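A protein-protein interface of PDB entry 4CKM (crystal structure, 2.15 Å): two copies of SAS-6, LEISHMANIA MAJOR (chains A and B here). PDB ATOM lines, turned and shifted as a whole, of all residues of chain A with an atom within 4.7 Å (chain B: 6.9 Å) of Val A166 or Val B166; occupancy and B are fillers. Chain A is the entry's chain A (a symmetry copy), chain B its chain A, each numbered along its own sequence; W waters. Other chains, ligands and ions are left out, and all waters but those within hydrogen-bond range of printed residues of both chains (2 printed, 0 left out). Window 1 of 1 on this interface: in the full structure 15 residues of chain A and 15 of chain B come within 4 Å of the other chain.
The backbone carbonyl oxygen (O) of His B168 is in hydrogen-bond range of the side-chain amino group (NZ) of Lys A164. The side-chain amino group of Lys A164 is in hydrogen-bond range of the backbone carbonyl oxygen of Leu B109, 3.2 Å away. NZ of Lys B164 is in hydrogen-bond range of O of His A168. N of Thr A165 lies within hydrogen-bond range of O of Glu B110 (3.0 Å).
The side-chain carboxylate (OE1) of Glu A159 sits at hydrogen-bond distance from a ring nitrogen (NE2) of His A168, 2.8 Å away. O of Val A157 sits at hydrogen-bond distance from N of His A168, at 2.9 Å. The side-chain hydroxyl of Thr B161 is in hydrogen-bond range of the backbone carbonyl oxygen of Lys B164 (2.9 Å). O of Val B157 sits at hydrogen-bond distance from N of His B168 (2.9 Å). The backbone carbonyl oxygen of Glu B159 lies within hydrogen-bond range of the backbone NH of Val B166, 2.6 Å away. The guanidinium group of Arg B156 lies within salt-bridge range of the side-chain carboxylate of Glu B167 (2.8 Å).
Glu B110 touches Lys A164 (O to CB, 3.2 Å). OH of Tyr B121 touches CD of Lys A164, at 3.2 Å. Thr A165 touches Leu B109. Val A166 touches Val B166 (CG1 to CG1, 3.4 Å). Val A166 touches Glu B167. Val A166 touches His B168 (CG2 to ND1, 3.8 Å). Val B166 touches Glu A167 (CG1 to O, 3.6 Å). ND1 of His A168 touches CG2 of Val B166, 3.8 Å away.
Thr A161 touches none of the printed residues of chain B. Printed residues of chain B within 4 Å of Thr A165: Leu B109 and Glu B110. Of chain B, only Val B166, Glu B167 and His B168 come within 4 Å of Val A166. Arg B156 touches none of the printed residues of chain A. Val B166 touches three residues of chain A. Of the printed residues of chain A, Glu B167 touches Val A166 (3.6 Å). The nearest printed residue of chain A that does not touch Val B166 is Glu A159 (6.0 Å). The nearest printed residue of chain B that does not touch Lys A164 is Ile B169 (4.2 Å).
Of the 16 printed residues of chain B, 7 touch a printed residue of chain A. Hydrophobic or aromatic side chains of chain B within 4 Å of the printed part of chain A: Tyr B121, Val B166 and His B168. Of the 9 printed residues of chain A, 5 touch a printed residue of chain B. Hydrophobic or aromatic side chains of chain A that line the printed part of chain B: Val A166 and His A168. Among the printed residues, 12 pairs touch across the chains. Among the printed residues, no Asp or Glu carboxylate lies within 4 Å of a Lys or Arg side-chain nitrogen of the other chain.
Lys A164 touches His B168, and with the chains exchanged His A168 touches Lys B164. Val B166 touches its own counterpart, Val A166. Val A166 touches Glu B167, and with the chains exchanged Glu A167 touches Val B166. Val A166 touches His B168, and with the chains exchanged His A168 touches Val B166. Of the 12 pairs that touch across the chains among the printed residues, 7 have their exchanged pair printed and touching as well.
Water W2 bridges NZ of Lys A164 (2.6 Å) and O of Leu B109 (3.1 Å). Water W1 bridges the side-chain carboxylate (OE2) of Glu B110 and the backbone carbonyl oxygen (O) of Thr A165.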
ATOM      1  N   VAL A 157      33.140 -29.007   2.015  1.00  0.00           N
ATOM      2  CA  VAL A 157      33.411 -27.609   2.278  1.00  0.00           C
ATOM      3  C   VAL A 157      32.216 -26.840   1.767  1.00  0.00           C
ATOM      4  O   VAL A 157      31.916 -26.882   0.575  1.00  0.00           O
ATOM      5  CB  VAL A 157      34.674 -27.113   1.555  1.00  0.00           C
ATOM      6  CG1 VAL A 157      34.890 -25.637   1.817  1.00  0.00           C
ATOM      7  CG2 VAL A 157      35.903 -27.888   2.007  1.00  0.00           C
ATOM      8  N   LEU A 158      31.537 -26.153   2.683  1.00  0.00           N
ATOM      9  CA  LEU A 158      30.244 -25.529   2.428  1.00  0.00           C
ATOM     10  C   LEU A 158      30.306 -24.025   2.607  1.00  0.00           C
ATOM     11  O   LEU A 158      31.062 -23.504   3.432  1.00  0.00           O
ATOM     12  CB  LEU A 158      29.202 -26.089   3.404  1.00  0.00           C
ATOM     13  CG  LEU A 158      29.082 -27.615   3.384  1.00  0.00           C
ATOM     14  CD1 LEU A 158      28.122 -28.078   4.475  1.00  0.00           C
ATOM     15  CD2 LEU A 158      28.646 -28.099   1.990  1.00  0.00           C
ATOM     16  N   GLU A 159      29.502 -23.332   1.822  1.00  0.00           N
ATOM     17  CA  GLU A 159      29.333 -21.889   1.943  1.00  0.00           C
ATOM     18  C   GLU A 159      27.852 -21.626   2.009  1.00  0.00           C
ATOM     19  O   GLU A 159      27.107 -22.083   1.148  1.00  0.00           O
ATOM     20  CB  GLU A 159      29.887 -21.179   0.713  1.00  0.00           C
ATOM     21  CG  GLU A 159      29.667 -19.670   0.719  1.00  0.00           C
ATOM     22  CD  GLU A 159      29.944 -18.998  -0.622  1.00  0.00           C
ATOM     23  OE1 GLU A 159      30.167 -19.689  -1.635  1.00  0.00           O
ATOM     24  OE2 GLU A 159      29.922 -17.756  -0.672  1.00  0.00           O
ATOM     25  N   THR A 161      25.032 -19.033   1.490  1.00  0.00           N
ATOM     26  CA  THR A 161      24.719 -17.749   0.887  1.00  0.00           C
ATOM     27  C   THR A 161      23.404 -17.300   1.485  1.00  0.00           C
ATOM     28  O   THR A 161      22.888 -17.953   2.392  1.00  0.00           O
ATOM     29  CB  THR A 161      24.586 -17.868  -0.634  1.00  0.00           C
ATOM     30  OG1 THR A 161      23.475 -18.705  -0.957  1.00  0.00           O
ATOM     31  CG2 THR A 161      25.864 -18.473  -1.240  1.00  0.00           C
ATOM     32  N   LYS A 164      21.017 -20.306  -0.015  1.00  0.00           N
ATOM     33  CA  LYS A 164      21.206 -21.723   0.312  1.00  0.00           C
ATOM     34  C   LYS A 164      22.632 -21.997   0.700  1.00  0.00           C
ATOM     35  O   LYS A 164      23.504 -21.147   0.530  1.00  0.00           O
ATOM     36  CB  LYS A 164      20.904 -22.603  -0.902  1.00  0.00           C
ATOM     37  CG  LYS A 164      21.951 -22.494  -2.005  1.00  0.00           C
ATOM     38  CD  LYS A 164      21.430 -22.993  -3.343  1.00  0.00           C
ATOM     39  CE  LYS A 164      21.147 -24.481  -3.352  1.00  0.00           C
ATOM     40  NZ  LYS A 164      22.377 -25.274  -3.125  1.00  0.00           N
ATOM     41  N   THR A 165      22.863 -23.225   1.142  1.00  0.00           N
ATOM     42  CA  THR A 165      24.197 -23.728   1.328  1.00  0.00           C
ATOM     43  C   THR A 165      24.701 -24.324   0.022  1.00  0.00           C
ATOM     44  O   THR A 165      24.020 -25.129  -0.631  1.00  0.00           O
ATOM     45  CB  THR A 165      24.267 -24.751   2.458  1.00  0.00           C
ATOM     46  OG1 THR A 165      23.903 -24.106   3.679  1.00  0.00           O
ATOM     47  CG2 THR A 165      25.673 -25.309   2.592  1.00  0.00           C
ATOM     48  N   VAL A 166      25.911 -23.912  -0.346  1.00  0.00           N
ATOM     49  CA  VAL A 166      26.537 -24.312  -1.602  1.00  0.00           C
ATOM     50  C   VAL A 166      27.745 -25.162  -1.288  1.00  0.00           C
ATOM     51  O   VAL A 166      28.629 -24.739  -0.533  1.00  0.00           O
ATOM     52  CB  VAL A 166      27.030 -23.070  -2.364  1.00  0.00           C
ATOM     53  CG1 VAL A 166      27.772 -23.471  -3.615  1.00  0.00           C
ATOM     54  CG2 VAL A 166      25.863 -22.177  -2.718  1.00  0.00           C
ATOM     55  N   GLU A 167      27.807 -26.339  -1.880  1.00  0.00           N
ATOM     56  CA  GLU A 167      28.952 -27.193  -1.712  1.00  0.00           C
ATOM     57  C   GLU A 167      30.063 -26.787  -2.696  1.00  0.00           C
ATOM     58  O   GLU A 167      29.832 -26.721  -3.892  1.00  0.00           O
ATOM     59  CB  GLU A 167      28.535 -28.623  -1.939  1.00  0.00           C
ATOM     60  CG  GLU A 167      29.674 -29.588  -1.778  1.00  0.00           C
ATOM     61  CD  GLU A 167      29.292 -30.953  -2.258  1.00  0.00           C
ATOM     62  OE1 GLU A 167      28.491 -31.617  -1.568  1.00  0.00           O
ATOM     63  OE2 GLU A 167      29.792 -31.340  -3.336  1.00  0.00           O
ATOM     64  N   HIS A 168      31.244 -26.472  -2.169  1.00  0.00           N
ATOM     65  CA  HIS A 168      32.407 -26.152  -2.976  1.00  0.00           C
ATOM     66  C   HIS A 168      33.136 -27.401  -3.377  1.00  0.00           C
ATOM     67  O   HIS A 168      33.493 -27.535  -4.522  1.00  0.00           O
ATOM     68  CB  HIS A 168      33.357 -25.185  -2.253  1.00  0.00           C
ATOM     69  CG  HIS A 168      32.917 -23.766  -2.362  1.00  0.00           C
ATOM     70  ND1 HIS A 168      33.553 -22.852  -3.164  1.00  0.00           N
ATOM     71  CD2 HIS A 168      31.839 -23.130  -1.842  1.00  0.00           C
ATOM     72  CE1 HIS A 168      32.910 -21.700  -3.111  1.00  0.00           C
ATOM     73  NE2 HIS A 168      31.864 -21.842  -2.317  1.00  0.00           N
ATOM     74  N   LEU B 109      18.150 -29.782  -1.046  1.00  0.00           N
ATOM     75  CA  LEU B 109      19.059 -28.801  -1.653  1.00  0.00           C
ATOM     76  C   LEU B 109      19.697 -27.799  -0.661  1.00  0.00           C
ATOM     77  O   LEU B 109      20.503 -26.930  -1.054  1.00  0.00           O
ATOM     78  CB  LEU B 109      18.314 -28.050  -2.748  1.00  0.00           C
ATOM     79  CG  LEU B 109      17.857 -28.916  -3.926  1.00  0.00           C
ATOM     80  CD1 LEU B 109      17.022 -28.079  -4.869  1.00  0.00           C
ATOM     81  CD2 LEU B 109      19.061 -29.484  -4.660  1.00  0.00           C
ATOM     82  N   GLU B 110      19.326 -27.903   0.614  1.00  0.00           N
ATOM     83  CA  GLU B 110      19.772 -26.959   1.645  1.00  0.00           C
ATOM     84  C   GLU B 110      19.412 -25.522   1.303  1.00  0.00           C
ATOM     85  O   GLU B 110      20.193 -24.586   1.472  1.00  0.00           O
ATOM     86  CB  GLU B 110      21.267 -27.139   1.944  1.00  0.00           C
ATOM     87  CG  GLU B 110      21.632 -28.614   2.133  1.00  0.00           C
ATOM     88  CD  GLU B 110      22.859 -28.877   2.993  1.00  0.00           C
ATOM     89  OE1 GLU B 110      23.310 -27.999   3.768  1.00  0.00           O
ATOM     90  OE2 GLU B 110      23.360 -30.008   2.921  1.00  0.00           O
ATOM     91  N   TYR B 121      14.233 -16.100  -6.157  1.00  0.00           N
ATOM     92  CA  TYR B 121      15.665 -16.313  -6.102  1.00  0.00           C
ATOM     93  C   TYR B 121      16.137 -16.884  -7.427  1.00  0.00           C
ATOM     94  O   TYR B 121      17.125 -16.449  -8.006  1.00  0.00           O
ATOM     95  CB  TYR B 121      15.992 -17.234  -4.908  1.00  0.00           C
ATOM     96  CG  TYR B 121      17.189 -18.168  -5.045  1.00  0.00           C
ATOM     97  CD1 TYR B 121      18.484 -17.662  -5.188  1.00  0.00           C
ATOM     98  CD2 TYR B 121      17.030 -19.573  -4.973  1.00  0.00           C
ATOM     99  CE1 TYR B 121      19.581 -18.517  -5.282  1.00  0.00           C
ATOM    100  CE2 TYR B 121      18.117 -20.430  -5.079  1.00  0.00           C
ATOM    101  CZ  TYR B 121      19.389 -19.895  -5.224  1.00  0.00           C
ATOM    102  OH  TYR B 121      20.484 -20.703  -5.316  1.00  0.00           O
ATOM    103  N   TYR B 136      27.626 -16.295 -13.390  1.00  0.00           N
ATOM    104  CA  TYR B 136      27.142 -17.648 -13.372  1.00  0.00           C
ATOM    105  C   TYR B 136      26.868 -18.108 -14.770  1.00  0.00           C
ATOM    106  O   TYR B 136      26.631 -17.303 -15.637  1.00  0.00           O
ATOM    107  CB  TYR B 136      25.842 -17.759 -12.546  1.00  0.00           C
ATOM    108  CG  TYR B 136      25.979 -17.491 -11.047  1.00  0.00           C
ATOM    109  CD1 TYR B 136      27.223 -17.386 -10.430  1.00  0.00           C
ATOM    110  CD2 TYR B 136      24.851 -17.374 -10.238  1.00  0.00           C
ATOM    111  CE1 TYR B 136      27.333 -17.151  -9.067  1.00  0.00           C
ATOM    112  CE2 TYR B 136      24.953 -17.139  -8.879  1.00  0.00           C
ATOM    113  CZ  TYR B 136      26.196 -17.032  -8.299  1.00  0.00           C
ATOM    114  OH  TYR B 136      26.309 -16.803  -6.948  1.00  0.00           O
ATOM    115  N   ARG B 156      21.748 -27.029 -14.457  1.00  0.00           N
ATOM    116  CA  ARG B 156      22.663 -26.624 -13.414  1.00  0.00           C
ATOM    117  C   ARG B 156      23.031 -25.134 -13.534  1.00  0.00           C
ATOM    118  O   ARG B 156      23.264 -24.619 -14.627  1.00  0.00           O
ATOM    119  CB  ARG B 156      23.928 -27.464 -13.500  1.00  0.00           C
ATOM    120  CG  ARG B 156      23.727 -28.957 -13.310  1.00  0.00           C
ATOM    121  CD  ARG B 156      24.986 -29.760 -13.654  1.00  0.00           C
ATOM    122  NE  ARG B 156      25.966 -29.728 -12.569  1.00  0.00           N
ATOM    123  CZ  ARG B 156      27.306 -29.710 -12.720  1.00  0.00           C
ATOM    124  NH1 ARG B 156      27.872 -29.724 -13.927  1.00  0.00           N
ATOM    125  NH2 ARG B 156      28.102 -29.653 -11.646  1.00  0.00           N
ATOM    126  N   VAL B 157      23.084 -24.445 -12.399  1.00  0.00           N
ATOM    127  CA  VAL B 157      23.582 -23.087 -12.325  1.00  0.00           C
ATOM    128  C   VAL B 157      24.968 -23.172 -11.731  1.00  0.00           C
ATOM    129  O   VAL B 157      25.130 -23.627 -10.599  1.00  0.00           O
ATOM    130  CB  VAL B 157      22.707 -22.192 -11.432  1.00  0.00           C
ATOM    131  CG1 VAL B 157      23.291 -20.798 -11.344  1.00  0.00           C
ATOM    132  CG2 VAL B 157      21.286 -22.108 -11.969  1.00  0.00           C
ATOM    133  N   LEU B 158      25.958 -22.744 -12.511  1.00  0.00           N
ATOM    134  CA  LEU B 158      27.369 -22.942 -12.203  1.00  0.00           C
ATOM    135  C   LEU B 158      28.095 -21.622 -12.039  1.00  0.00           C
ATOM    136  O   LEU B 158      27.763 -20.619 -12.677  1.00  0.00           O
ATOM    137  CB  LEU B 158      28.038 -23.721 -13.343  1.00  0.00           C
ATOM    138  CG  LEU B 158      27.361 -25.054 -13.672  1.00  0.00           C
ATOM    139  CD1 LEU B 158      28.017 -25.685 -14.896  1.00  0.00           C
ATOM    140  CD2 LEU B 158      27.402 -25.990 -12.451  1.00  0.00           C
ATOM    141  N   GLU B 159      29.089 -21.632 -11.170  1.00  0.00           N
ATOM    142  CA  GLU B 159      29.978 -20.493 -10.976  1.00  0.00           C
ATOM    143  C   GLU B 159      31.387 -21.015 -11.073  1.00  0.00           C
ATOM    144  O   GLU B 159      31.739 -21.968 -10.384  1.00  0.00           O
ATOM    145  CB  GLU B 159      29.789 -19.895  -9.586  1.00  0.00           C
ATOM    146  CG  GLU B 159      30.748 -18.754  -9.269  1.00  0.00           C
ATOM    147  CD  GLU B 159      30.770 -18.353  -7.797  1.00  0.00           C
ATOM    148  OE1 GLU B 159      30.162 -19.039  -6.952  1.00  0.00           O
ATOM    149  OE2 GLU B 159      31.420 -17.344  -7.472  1.00  0.00           O
ATOM    150  N   THR B 160      32.191 -20.408 -11.921  1.00  0.00           N
ATOM    151  CA  THR B 160      33.581 -20.797 -12.029  1.00  0.00           C
ATOM    152  C   THR B 160      34.415 -19.868 -11.161  1.00  0.00           C
ATOM    153  O   THR B 160      34.394 -18.683 -11.353  1.00  0.00           O
ATOM    154  CB  THR B 160      34.046 -20.808 -13.495  1.00  0.00           C
ATOM    155  OG1 THR B 160      33.436 -21.929 -14.170  1.00  0.00           O
ATOM    156  CG2 THR B 160      35.545 -21.012 -13.576  1.00  0.00           C
ATOM    157  N   THR B 161      35.096 -20.417 -10.165  1.00  0.00           N
ATOM    158  CA  THR B 161      35.982 -19.644  -9.312  1.00  0.00           C
ATOM    159  C   THR B 161      37.377 -19.809  -9.875  1.00  0.00           C
ATOM    160  O   THR B 161      37.542 -20.413 -10.935  1.00  0.00           O
ATOM    161  CB  THR B 161      35.941 -20.151  -7.866  1.00  0.00           C
ATOM    162  OG1 THR B 161      36.446 -21.486  -7.808  1.00  0.00           O
ATOM    163  CG2 THR B 161      34.499 -20.137  -7.333  1.00  0.00           C
ATOM    164  N   LYS B 164      37.797 -23.859  -9.235  1.00  0.00           N
ATOM    165  CA  LYS B 164      36.932 -24.867  -9.858  1.00  0.00           C
ATOM    166  C   LYS B 164      35.593 -24.280 -10.208  1.00  0.00           C
ATOM    167  O   LYS B 164      35.269 -23.167  -9.798  1.00  0.00           O
ATOM    168  CB  LYS B 164      36.666 -26.022  -8.892  1.00  0.00           C
ATOM    169  CG  LYS B 164      35.755 -25.644  -7.730  1.00  0.00           C
ATOM    170  CD  LYS B 164      35.865 -26.623  -6.573  1.00  0.00           C
ATOM    171  CE  LYS B 164      35.347 -28.005  -6.913  1.00  0.00           C
ATOM    172  NZ  LYS B 164      33.902 -27.985  -7.235  1.00  0.00           N
ATOM    173  N   THR B 165      34.796 -25.083 -10.898  1.00  0.00           N
ATOM    174  CA  THR B 165      33.407 -24.778 -11.107  1.00  0.00           C
ATOM    175  C   THR B 165      32.589 -25.308  -9.940  1.00  0.00           C
ATOM    176  O   THR B 165      32.722 -26.470  -9.527  1.00  0.00           O
ATOM    177  CB  THR B 165      32.895 -25.340 -12.431  1.00  0.00           C
ATOM    178  OG1 THR B 165      33.613 -24.717 -13.497  1.00  0.00           O
ATOM    179  CG2 THR B 165      31.412 -25.056 -12.599  1.00  0.00           C
ATOM    180  N   VAL B 166      31.739 -24.430  -9.414  1.00  0.00           N
ATOM    181  CA  VAL B 166      30.919 -24.724  -8.242  1.00  0.00           C
ATOM    182  C   VAL B 166      29.469 -24.742  -8.663  1.00  0.00           C
ATOM    183  O   VAL B 166      28.973 -23.772  -9.248  1.00  0.00           O
ATOM    184  CB  VAL B 166      31.083 -23.611  -7.194  1.00  0.00           C
ATOM    185  CG1 VAL B 166      30.163 -23.844  -6.020  1.00  0.00           C
ATOM    186  CG2 VAL B 166      32.517 -23.543  -6.722  1.00  0.00           C
ATOM    187  N   GLU B 167      28.778 -25.821  -8.346  1.00  0.00           N
ATOM    188  CA  GLU B 167      27.371 -25.908  -8.629  1.00  0.00           C
ATOM    189  C   GLU B 167      26.564 -25.224  -7.512  1.00  0.00           C
ATOM    190  O   GLU B 167      26.721 -25.554  -6.348  1.00  0.00           O
ATOM    191  CB  GLU B 167      26.984 -27.359  -8.754  1.00  0.00           C
ATOM    192  CG  GLU B 167      25.525 -27.544  -9.055  1.00  0.00           C
ATOM    193  CD  GLU B 167      25.127 -28.979  -8.916  1.00  0.00           C
ATOM    194  OE1 GLU B 167      25.517 -29.785  -9.785  1.00  0.00           O
ATOM    195  OE2 GLU B 167      24.433 -29.286  -7.922  1.00  0.00           O
ATOM    196  N   HIS B 168      25.744 -24.242  -7.881  1.00  0.00           N
ATOM    197  CA  HIS B 168      24.860 -23.563  -6.951  1.00  0.00           C
ATOM    198  C   HIS B 168      23.572 -24.317  -6.794  1.00  0.00           C
ATOM    199  O   HIS B 168      23.126 -24.502  -5.689  1.00  0.00           O
ATOM    200  CB  HIS B 168      24.583 -22.114  -7.379  1.00  0.00           C
ATOM    201  CG  HIS B 168      25.678 -21.184  -6.984  1.00  0.00           C
ATOM    202  ND1 HIS B 168      25.549 -20.279  -5.960  1.00  0.00           N
ATOM    203  CD2 HIS B 168      26.960 -21.090  -7.415  1.00  0.00           C
ATOM    204  CE1 HIS B 168      26.692 -19.639  -5.794  1.00  0.00           C
ATOM    205  NE2 HIS B 168      27.566 -20.113  -6.664  1.00  0.00           N
ATOM    206  N   ILE B 169      22.978 -24.776  -7.889  1.00  0.00           N
ATOM    207  CA  ILE B 169      21.755 -25.575  -7.788  1.00  0.00           C
ATOM    208  C   ILE B 169      21.603 -26.423  -9.025  1.00  0.00           C
ATOM    209  O   ILE B 169      22.156 -26.095 -10.074  1.00  0.00           O
ATOM    210  CB  ILE B 169      20.535 -24.666  -7.543  1.00  0.00           C
ATOM    211  CG1 ILE B 169      19.277 -25.474  -7.203  1.00  0.00           C
ATOM    212  CG2 ILE B 169      20.264 -23.740  -8.719  1.00  0.00           C
ATOM    213  CD1 ILE B 169      18.126 -24.565  -6.813  1.00  0.00           C
HETATM  214  O   HOH W   1      24.434 -28.358   0.308  1.00  0.00           O
HETATM  215  O   HOH W   2      22.378 -27.907  -3.268  1.00  0.00           O
